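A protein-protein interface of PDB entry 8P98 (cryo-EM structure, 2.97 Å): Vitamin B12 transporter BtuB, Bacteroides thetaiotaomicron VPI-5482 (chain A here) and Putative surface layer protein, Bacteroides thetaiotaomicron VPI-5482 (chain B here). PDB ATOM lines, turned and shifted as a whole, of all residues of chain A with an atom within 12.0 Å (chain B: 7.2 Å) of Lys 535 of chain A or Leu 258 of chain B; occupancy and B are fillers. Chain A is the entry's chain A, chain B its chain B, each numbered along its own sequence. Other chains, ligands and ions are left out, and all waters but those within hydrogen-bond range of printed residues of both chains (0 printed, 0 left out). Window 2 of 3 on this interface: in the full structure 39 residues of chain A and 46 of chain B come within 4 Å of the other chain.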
ATOM      1  N   LEU A 482       5.009   6.083 -22.359  1.00  0.00           N
ATOM      2  CA  LEU A 482       4.316   7.348 -22.113  1.00  0.00           C
ATOM      3  C   LEU A 482       2.857   7.368 -22.557  1.00  0.00           C
ATOM      4  O   LEU A 482       2.005   7.786 -21.757  1.00  0.00           O
ATOM      5  CB  LEU A 482       5.108   8.489 -22.769  1.00  0.00           C
ATOM      6  CG  LEU A 482       4.550   9.896 -22.550  1.00  0.00           C
ATOM      7  CD1 LEU A 482       4.567  10.248 -21.072  1.00  0.00           C
ATOM      8  CD2 LEU A 482       5.334  10.919 -23.356  1.00  0.00           C
ATOM      9  N   PRO A 483       2.487   6.944 -23.772  1.00  0.00           N
ATOM     10  CA  PRO A 483       1.065   6.981 -24.138  1.00  0.00           C
ATOM     11  C   PRO A 483       0.259   5.787 -23.650  1.00  0.00           C
ATOM     12  O   PRO A 483      -0.973   5.818 -23.759  1.00  0.00           O
ATOM     13  CB  PRO A 483       1.103   7.027 -25.669  1.00  0.00           C
ATOM     14  CG  PRO A 483       2.333   6.312 -26.021  1.00  0.00           C
ATOM     15  CD  PRO A 483       3.330   6.579 -24.926  1.00  0.00           C
ATOM     16  N   GLY A 484       0.898   4.745 -23.122  1.00  0.00           N
ATOM     17  CA  GLY A 484       0.162   3.572 -22.688  1.00  0.00           C
ATOM     18  C   GLY A 484       0.674   2.906 -21.427  1.00  0.00           C
ATOM     19  O   GLY A 484       0.468   1.705 -21.232  1.00  0.00           O
ATOM     20  N   GLY A 485       1.340   3.664 -20.561  1.00  0.00           N
ATOM     21  CA  GLY A 485       1.926   3.084 -19.369  1.00  0.00           C
ATOM     22  C   GLY A 485       0.984   3.001 -18.186  1.00  0.00           C
ATOM     23  O   GLY A 485       0.371   4.000 -17.796  1.00  0.00           O
ATOM     24  N   LEU A 531      -2.970  -4.885 -25.046  1.00  0.00           N
ATOM     25  CA  LEU A 531      -4.251  -4.901 -25.730  1.00  0.00           C
ATOM     26  C   LEU A 531      -4.712  -3.474 -25.982  1.00  0.00           C
ATOM     27  O   LEU A 531      -4.374  -2.564 -25.216  1.00  0.00           O
ATOM     28  CB  LEU A 531      -5.312  -5.654 -24.913  1.00  0.00           C
ATOM     29  CG  LEU A 531      -5.274  -7.175 -25.065  1.00  0.00           C
ATOM     30  CD1 LEU A 531      -6.426  -7.825 -24.321  1.00  0.00           C
ATOM     31  CD2 LEU A 531      -5.295  -7.562 -26.534  1.00  0.00           C
ATOM     32  N   PRO A 532      -5.477  -3.249 -27.048  1.00  0.00           N
ATOM     33  CA  PRO A 532      -5.974  -1.899 -27.325  1.00  0.00           C
ATOM     34  C   PRO A 532      -6.967  -1.437 -26.272  1.00  0.00           C
ATOM     35  O   PRO A 532      -7.666  -2.236 -25.645  1.00  0.00           O
ATOM     36  CB  PRO A 532      -6.648  -2.040 -28.694  1.00  0.00           C
ATOM     37  CG  PRO A 532      -6.989  -3.485 -28.797  1.00  0.00           C
ATOM     38  CD  PRO A 532      -5.904  -4.218 -28.071  1.00  0.00           C
ATOM     39  N   THR A 533      -7.018  -0.124 -26.081  1.00  0.00           N
ATOM     40  CA  THR A 533      -7.936   0.500 -25.147  1.00  0.00           C
ATOM     41  C   THR A 533      -8.993   1.290 -25.904  1.00  0.00           C
ATOM     42  O   THR A 533      -8.808   1.664 -27.065  1.00  0.00           O
ATOM     43  CB  THR A 533      -7.196   1.423 -24.176  1.00  0.00           C
ATOM     44  OG1 THR A 533      -6.468   2.408 -24.919  1.00  0.00           O
ATOM     45  CG2 THR A 533      -6.230   0.623 -23.323  1.00  0.00           C
ATOM     46  N   SER A 534     -10.114   1.538 -25.225  1.00  0.00           N
ATOM     47  CA  SER A 534     -11.204   2.283 -25.847  1.00  0.00           C
ATOM     48  C   SER A 534     -10.783   3.701 -26.203  1.00  0.00           C
ATOM     49  O   SER A 534     -11.309   4.282 -27.159  1.00  0.00           O
ATOM     50  CB  SER A 534     -12.418   2.307 -24.921  1.00  0.00           C
ATOM     51  OG  SER A 534     -12.110   2.946 -23.695  1.00  0.00           O
ATOM     52  N   LYS A 535      -9.839   4.274 -25.453  1.00  0.00           N
ATOM     53  CA  LYS A 535      -9.382   5.625 -25.757  1.00  0.00           C
ATOM     54  C   LYS A 535      -8.635   5.681 -27.082  1.00  0.00           C
ATOM     55  O   LYS A 535      -8.731   6.680 -27.802  1.00  0.00           O
ATOM     56  CB  LYS A 535      -8.498   6.155 -24.630  1.00  0.00           C
ATOM     57  CG  LYS A 535      -8.158   7.624 -24.779  1.00  0.00           C
ATOM     58  CD  LYS A 535      -9.397   8.481 -24.589  1.00  0.00           C
ATOM     59  CE  LYS A 535      -9.073   9.958 -24.695  1.00  0.00           C
ATOM     60  NZ  LYS A 535      -8.714  10.331 -26.088  1.00  0.00           N
ATOM     61  N   GLY A 536      -7.894   4.630 -27.421  1.00  0.00           N
ATOM     62  CA  GLY A 536      -7.170   4.600 -28.676  1.00  0.00           C
ATOM     63  C   GLY A 536      -5.683   4.352 -28.537  1.00  0.00           C
ATOM     64  O   GLY A 536      -4.901   4.734 -29.412  1.00  0.00           O
ATOM     65  N   PHE A 537      -5.275   3.715 -27.441  1.00  0.00           N
ATOM     66  CA  PHE A 537      -3.884   3.345 -27.236  1.00  0.00           C
ATOM     67  C   PHE A 537      -3.822   1.946 -26.643  1.00  0.00           C
ATOM     68  O   PHE A 537      -4.847   1.314 -26.372  1.00  0.00           O
ATOM     69  CB  PHE A 537      -3.152   4.361 -26.346  1.00  0.00           C
ATOM     70  CG  PHE A 537      -3.692   4.452 -24.947  1.00  0.00           C
ATOM     71  CD1 PHE A 537      -4.708   5.342 -24.642  1.00  0.00           C
ATOM     72  CD2 PHE A 537      -3.172   3.663 -23.935  1.00  0.00           C
ATOM     73  CE1 PHE A 537      -5.205   5.435 -23.357  1.00  0.00           C
ATOM     74  CE2 PHE A 537      -3.664   3.751 -22.647  1.00  0.00           C
ATOM     75  CZ  PHE A 537      -4.683   4.639 -22.358  1.00  0.00           C
ATOM     76  N   TYR A 538      -2.601   1.461 -26.451  1.00  0.00           N
ATOM     77  CA  TYR A 538      -2.358   0.104 -25.985  1.00  0.00           C
ATOM     78  C   TYR A 538      -2.010   0.105 -24.504  1.00  0.00           C
ATOM     79  O   TYR A 538      -1.320   1.006 -24.018  1.00  0.00           O
ATOM     80  CB  TYR A 538      -1.227  -0.542 -26.784  1.00  0.00           C
ATOM     81  CG  TYR A 538      -1.694  -1.320 -27.988  1.00  0.00           C
ATOM     82  CD1 TYR A 538      -2.866  -0.979 -28.647  1.00  0.00           C
ATOM     83  CD2 TYR A 538      -0.968  -2.404 -28.458  1.00  0.00           C
ATOM     84  CE1 TYR A 538      -3.295  -1.689 -29.744  1.00  0.00           C
ATOM     85  CE2 TYR A 538      -1.392  -3.120 -29.554  1.00  0.00           C
ATOM     86  CZ  TYR A 538      -2.555  -2.760 -30.192  1.00  0.00           C
ATOM     87  OH  TYR A 538      -2.977  -3.476 -31.285  1.00  0.00           O
ATOM     88  N   SER A 539      -2.488  -0.914 -23.786  1.00  0.00           N
ATOM     89  CA  SER A 539      -2.218  -1.022 -22.364  1.00  0.00           C
ATOM     90  C   SER A 539      -2.324  -2.476 -21.924  1.00  0.00           C
ATOM     91  O   SER A 539      -3.330  -3.130 -22.234  1.00  0.00           O
ATOM     92  CB  SER A 539      -3.180  -0.162 -21.547  1.00  0.00           C
ATOM     93  OG  SER A 539      -2.935  -0.300 -20.159  1.00  0.00           O
ATOM     94  N   PRO A 540      -1.322  -3.000 -21.222  1.00  0.00           N
ATOM     95  CA  PRO A 540      -1.399  -4.384 -20.739  1.00  0.00           C
ATOM     96  C   PRO A 540      -2.517  -4.565 -19.724  1.00  0.00           C
ATOM     97  O   PRO A 540      -2.796  -3.676 -18.917  1.00  0.00           O
ATOM     98  CB  PRO A 540      -0.026  -4.610 -20.099  1.00  0.00           C
ATOM     99  CG  PRO A 540       0.468  -3.236 -19.776  1.00  0.00           C
ATOM    100  CD  PRO A 540      -0.048  -2.358 -20.866  1.00  0.00           C
ATOM    101  N   VAL A 541      -3.161  -5.730 -19.770  1.00  0.00           N
ATOM    102  CA  VAL A 541      -4.298  -5.992 -18.895  1.00  0.00           C
ATOM    103  C   VAL A 541      -4.189  -7.349 -18.206  1.00  0.00           C
ATOM    104  O   VAL A 541      -5.202  -7.910 -17.776  1.00  0.00           O
ATOM    105  CB  VAL A 541      -5.619  -5.890 -19.678  1.00  0.00           C
ATOM    106  CG1 VAL A 541      -5.914  -4.444 -20.033  1.00  0.00           C
ATOM    107  CG2 VAL A 541      -5.552  -6.740 -20.929  1.00  0.00           C
ATOM    108  N   GLY B 226      -8.352  12.567 -34.031  1.00  0.00           N
ATOM    109  CA  GLY B 226      -7.512  13.267 -33.077  1.00  0.00           C
ATOM    110  C   GLY B 226      -6.077  12.807 -33.204  1.00  0.00           C
ATOM    111  O   GLY B 226      -5.200  13.570 -33.616  1.00  0.00           O
ATOM    112  N   GLY B 227      -5.827  11.555 -32.838  1.00  0.00           N
ATOM    113  CA  GLY B 227      -4.618  10.883 -33.260  1.00  0.00           C
ATOM    114  C   GLY B 227      -3.486  10.817 -32.261  1.00  0.00           C
ATOM    115  O   GLY B 227      -2.747  11.791 -32.090  1.00  0.00           O
ATOM    116  N   LYS B 229      -2.462  10.470 -28.852  1.00  0.00           N
ATOM    117  CA  LYS B 229      -2.169  11.461 -27.824  1.00  0.00           C
ATOM    118  C   LYS B 229      -0.712  11.352 -27.390  1.00  0.00           C
ATOM    119  O   LYS B 229      -0.205  10.260 -27.122  1.00  0.00           O
ATOM    120  CB  LYS B 229      -3.126  11.297 -26.636  1.00  0.00           C
ATOM    121  CG  LYS B 229      -3.031   9.997 -25.844  1.00  0.00           C
ATOM    122  CD  LYS B 229      -2.064  10.125 -24.673  1.00  0.00           C
ATOM    123  CE  LYS B 229      -2.050   8.873 -23.819  1.00  0.00           C
ATOM    124  NZ  LYS B 229      -1.091   8.998 -22.688  1.00  0.00           N
ATOM    125  N   TYR B 235      -2.213  16.537 -30.443  1.00  0.00           N
ATOM    126  CA  TYR B 235      -3.383  15.759 -30.066  1.00  0.00           C
ATOM    127  C   TYR B 235      -4.566  16.688 -29.854  1.00  0.00           C
ATOM    128  O   TYR B 235      -4.435  17.741 -29.223  1.00  0.00           O
ATOM    129  CB  TYR B 235      -3.103  14.935 -28.809  1.00  0.00           C
ATOM    130  CG  TYR B 235      -4.300  14.212 -28.258  1.00  0.00           C
ATOM    131  CD1 TYR B 235      -4.913  13.197 -28.974  1.00  0.00           C
ATOM    132  CD2 TYR B 235      -4.790  14.511 -26.998  1.00  0.00           C
ATOM    133  CE1 TYR B 235      -6.001  12.522 -28.464  1.00  0.00           C
ATOM    134  CE2 TYR B 235      -5.873  13.839 -26.478  1.00  0.00           C
ATOM    135  CZ  TYR B 235      -6.477  12.847 -27.215  1.00  0.00           C
ATOM    136  OH  TYR B 235      -7.560  12.175 -26.702  1.00  0.00           O
ATOM    137  N   GLU B 236      -5.720  16.293 -30.383  1.00  0.00           N
ATOM    138  CA  GLU B 236      -6.876  17.175 -30.436  1.00  0.00           C
ATOM    139  C   GLU B 236      -8.143  16.339 -30.350  1.00  0.00           C
ATOM    140  O   GLU B 236      -8.126  15.126 -30.571  1.00  0.00           O
ATOM    141  CB  GLU B 236      -6.861  18.018 -31.721  1.00  0.00           C
ATOM    142  CG  GLU B 236      -7.924  19.102 -31.800  1.00  0.00           C
ATOM    143  CD  GLU B 236      -7.848  19.899 -33.083  1.00  0.00           C
ATOM    144  OE1 GLU B 236      -6.987  19.584 -33.929  1.00  0.00           O
ATOM    145  OE2 GLU B 236      -8.650  20.840 -33.245  1.00  0.00           O
ATOM    146  N   GLU B 237      -9.240  16.997 -30.004  1.00  0.00           N
ATOM    147  CA  GLU B 237     -10.548  16.357 -30.040  1.00  0.00           C
ATOM    148  C   GLU B 237     -10.932  16.054 -31.482  1.00  0.00           C
ATOM    149  O   GLU B 237     -10.942  16.971 -32.315  1.00  0.00           O
ATOM    150  CB  GLU B 237     -11.593  17.260 -29.395  1.00  0.00           C
ATOM    151  CG  GLU B 237     -11.274  17.665 -27.971  1.00  0.00           C
ATOM    152  CD  GLU B 237     -12.515  17.779 -27.111  1.00  0.00           C
ATOM    153  OE1 GLU B 237     -13.540  18.284 -27.613  1.00  0.00           O
ATOM    154  OE2 GLU B 237     -12.468  17.362 -25.935  1.00  0.00           O
ATOM    155  N   PRO B 238     -11.242  14.805 -31.827  1.00  0.00           N
ATOM    156  CA  PRO B 238     -11.680  14.508 -33.195  1.00  0.00           C
ATOM    157  C   PRO B 238     -12.962  15.248 -33.539  1.00  0.00           C
ATOM    158  O   PRO B 238     -13.802  15.515 -32.678  1.00  0.00           O
ATOM    159  CB  PRO B 238     -11.897  12.990 -33.184  1.00  0.00           C
ATOM    160  CG  PRO B 238     -11.852  12.579 -31.745  1.00  0.00           C
ATOM    161  CD  PRO B 238     -11.011  13.584 -31.042  1.00  0.00           C
ATOM    162  N   LYS B 255     -18.328  18.107 -33.281  1.00  0.00           N
ATOM    163  CA  LYS B 255     -17.308  17.728 -32.313  1.00  0.00           C
ATOM    164  C   LYS B 255     -17.657  16.386 -31.686  1.00  0.00           C
ATOM    165  O   LYS B 255     -18.813  16.137 -31.331  1.00  0.00           O
ATOM    166  CB  LYS B 255     -17.164  18.785 -31.216  1.00  0.00           C
ATOM    167  CG  LYS B 255     -17.040  20.210 -31.724  1.00  0.00           C
ATOM    168  CD  LYS B 255     -15.805  20.378 -32.587  1.00  0.00           C
ATOM    169  CE  LYS B 255     -15.263  21.793 -32.495  1.00  0.00           C
ATOM    170  NZ  LYS B 255     -14.037  21.974 -33.317  1.00  0.00           N
ATOM    171  N   PHE B 256     -16.651  15.525 -31.549  1.00  0.00           N
ATOM    172  CA  PHE B 256     -16.853  14.212 -30.949  1.00  0.00           C
ATOM    173  C   PHE B 256     -15.965  14.038 -29.726  1.00  0.00           C
ATOM    174  O   PHE B 256     -15.304  13.006 -29.578  1.00  0.00           O
ATOM    175  CB  PHE B 256     -16.576  13.106 -31.965  1.00  0.00           C
ATOM    176  CG  PHE B 256     -17.480  13.145 -33.155  1.00  0.00           C
ATOM    177  CD1 PHE B 256     -18.834  13.376 -33.003  1.00  0.00           C
ATOM    178  CD2 PHE B 256     -16.979  12.948 -34.426  1.00  0.00           C
ATOM    179  CE1 PHE B 256     -19.669  13.415 -34.097  1.00  0.00           C
ATOM    180  CE2 PHE B 256     -17.811  12.983 -35.523  1.00  0.00           C
ATOM    181  CZ  PHE B 256     -19.159  13.218 -35.358  1.00  0.00           C
ATOM    182  N   GLN B 257     -15.928  15.064 -28.873  1.00  0.00           N
ATOM    183  CA  GLN B 257     -15.184  15.097 -27.614  1.00  0.00           C
ATOM    184  C   GLN B 257     -13.739  14.644 -27.793  1.00  0.00           C
ATOM    185  O   GLN B 257     -13.210  14.661 -28.908  1.00  0.00           O
ATOM    186  CB  GLN B 257     -15.897  14.275 -26.527  1.00  0.00           C
ATOM    187  CG  GLN B 257     -15.863  12.757 -26.663  1.00  0.00           C
ATOM    188  CD  GLN B 257     -16.650  12.060 -25.572  1.00  0.00           C
ATOM    189  OE1 GLN B 257     -17.171  12.702 -24.661  1.00  0.00           O
ATOM    190  NE2 GLN B 257     -16.743  10.738 -25.662  1.00  0.00           N
ATOM    191  N   LEU B 258     -13.091  14.235 -26.703  1.00  0.00           N
ATOM    192  CA  LEU B 258     -11.667  13.935 -26.731  1.00  0.00           C
ATOM    193  C   LEU B 258     -11.364  12.455 -26.909  1.00  0.00           C
ATOM    194  O   LEU B 258     -10.264  12.113 -27.360  1.00  0.00           O
ATOM    195  CB  LEU B 258     -11.001  14.439 -25.445  1.00  0.00           C
ATOM    196  CG  LEU B 258      -9.475  14.422 -25.407  1.00  0.00           C
ATOM    197  CD1 LEU B 258      -8.933  15.373 -26.456  1.00  0.00           C
ATOM    198  CD2 LEU B 258      -8.961  14.789 -24.028  1.00  0.00           C
ATOM    199  N   GLY B 259     -12.301  11.572 -26.576  1.00  0.00           N
ATOM    200  CA  GLY B 259     -12.058  10.153 -26.709  1.00  0.00           C
ATOM    201  C   GLY B 259     -12.265   9.634 -28.121  1.00  0.00           C
ATOM    202  O   GLY B 259     -12.860  10.289 -28.977  1.00  0.00           O
ATOM    203  N   ASP B 260     -11.737   8.428 -28.347  1.00  0.00           N
ATOM    204  CA  ASP B 260     -11.952   7.650 -29.564  1.00  0.00           C
ATOM    205  C   ASP B 260     -11.298   8.244 -30.807  1.00  0.00           C
ATOM    206  O   ASP B 260     -10.962   9.432 -30.846  1.00  0.00           O
ATOM    207  CB  ASP B 260     -13.447   7.451 -29.813  1.00  0.00           C
ATOM    208  CG  ASP B 260     -13.739   6.164 -30.542  1.00  0.00           C
ATOM    209  OD1 ASP B 260     -14.596   6.171 -31.448  1.00  0.00           O
ATOM    210  OD2 ASP B 260     -13.082   5.149 -30.229  1.00  0.00           O
ATOM    211  N   ALA B 261     -11.116   7.404 -31.830  1.00  0.00           N
ATOM    212  CA  ALA B 261     -10.462   7.769 -33.085  1.00  0.00           C
ATOM    213  C   ALA B 261     -11.381   7.414 -34.248  1.00  0.00           C
ATOM    214  O   ALA B 261     -11.349   6.283 -34.755  1.00  0.00           O
ATOM    215  CB  ALA B 261      -9.114   7.066 -33.219  1.00  0.00           C
ATOM    216  N   LYS B 279     -16.379   4.117 -32.792  1.00  0.00           N
ATOM    217  CA  LYS B 279     -16.895   3.026 -31.966  1.00  0.00           C
ATOM    218  C   LYS B 279     -18.285   2.617 -32.428  1.00  0.00           C
ATOM    219  O   LYS B 279     -18.456   1.608 -33.118  1.00  0.00           O
ATOM    220  CB  LYS B 279     -16.955   3.405 -30.484  1.00  0.00           C
ATOM    221  CG  LYS B 279     -15.632   3.490 -29.773  1.00  0.00           C
ATOM    222  CD  LYS B 279     -15.848   3.897 -28.324  1.00  0.00           C
ATOM    223  CE  LYS B 279     -14.535   4.057 -27.582  1.00  0.00           C
ATOM    224  NZ  LYS B 279     -14.750   4.485 -26.173  1.00  0.00           N
ATOM    225  N   TYR B 299     -21.281  -1.257 -30.600  1.00  0.00           N
ATOM    226  CA  TYR B 299     -19.842  -1.408 -30.366  1.00  0.00           C
ATOM    227  C   TYR B 299     -19.603  -2.354 -29.185  1.00  0.00           C
ATOM    228  O   TYR B 299     -19.141  -1.976 -28.109  1.00  0.00           O
ATOM    229  CB  TYR B 299     -19.164  -0.047 -30.155  1.00  0.00           C
ATOM    230  CG  TYR B 299     -17.668  -0.123 -29.954  1.00  0.00           C
ATOM    231  CD1 TYR B 299     -16.821  -0.355 -31.028  1.00  0.00           C
ATOM    232  CD2 TYR B 299     -17.101   0.055 -28.699  1.00  0.00           C
ATOM    233  CE1 TYR B 299     -15.456  -0.420 -30.859  1.00  0.00           C
ATOM    234  CE2 TYR B 299     -15.735  -0.011 -28.519  1.00  0.00           C
ATOM    235  CZ  TYR B 299     -14.916  -0.249 -29.604  1.00  0.00           C
ATOM    236  OH  TYR B 299     -13.553  -0.314 -29.433  1.00  0.00           O
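O of Leu 482 of chain A is in hydrogen-bond range of NZ of Lys 229 of chain B (3.5 Å). The backbone carbonyl oxygen (O) of Pro 483 of chain A sits close to the side-chain amino group (NZ) of Lys 229 of chain B (3.4 Å). NZ of Lys 535 of chain A sits at hydrogen-bond distance from O of Leu 258 of chain B (2.7 Å). The side-chain hydroxyl (OH) of Tyr 235 of chain B lies close to the side-chain amino group (NZ) of Lys 535 of chain A, 2.3 Å away.
Among the printed residues, merely in contact across the chains: Ser 534 of chain A with Lys 279 of chain B (3.3 Å), Lys 535 of chain A with Gly 259 of chain B (3.4 Å), Lys 535 of chain A with Asp 260 of chain B (3.5 Å) and Ser 534 of chain A with Asp 260 of chain B (3.6 Å).
Of the 16 printed residues of chain B, 6 touch a printed residue of chain A. Hydrophobic or aromatic side chains of chain B within 4 Å of the printed part of chain A: Tyr 235. Along chain B the printed residues that touch a printed residue of chain A span positions 229 to 279. Hydrophobic or aromatic side chains of chain A within 4 Å of the printed part of chain B: Pro 483. Among the printed residues, no Asp or Glu carboxylate lies within 4 Å of a Lys or Arg side-chain nitrogen of the other chain.
Of chain B, only Tyr 235, Leu 258, Gly 259 and Asp 260 come within 4 Å of Lys 535 of chain A. Leu 258 of chain B touches one residue of chain A. No residue of chain A comes within 4 Å of Pro 238 of chain B. No residue of chain A comes within 4 Å of Gln 257 of chain B. Asp 260 of chain B touches just these residues of chain A: Ser 534 (3.6 Å) and Lys 535 (3.5 Å). Ala 261 of chain B touches none of the printed residues of chain A. Printed residues of chain B within 4 Å of Ser 534 of chain A: Asp 260 (3.6 Å) and Lys 279 (3.3 Å). Printed residues of chain B within 4 Å of Leu 482 of chain A: Lys 229 (3.5 Å). Printed residues of chain A within 4 Å of Lys 279 of chain B: Ser 534. The nearest residue of chain B that does not touch Lys 535 of chain A is Ala 261 of chain B (4.7 Å). The nearest printed residue of chain A that does not touch Lys 229 of chain B is Phe 537 of chain A (4.5 Å).
OH of Tyr 235 of chain B sits at hydrogen-bond distance from O of Leu 258 of chain B, at 2.8 Å. The side-chain carboxylate (OE2) of Glu 237 of chain B lies within hydrogen-bond range of the backbone NH (N) of Leu 258 of chain B. OD1 of Asp 260 of chain B lies within hydrogen-bond range of N of Lys 279 of chain B (3.0 Å).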
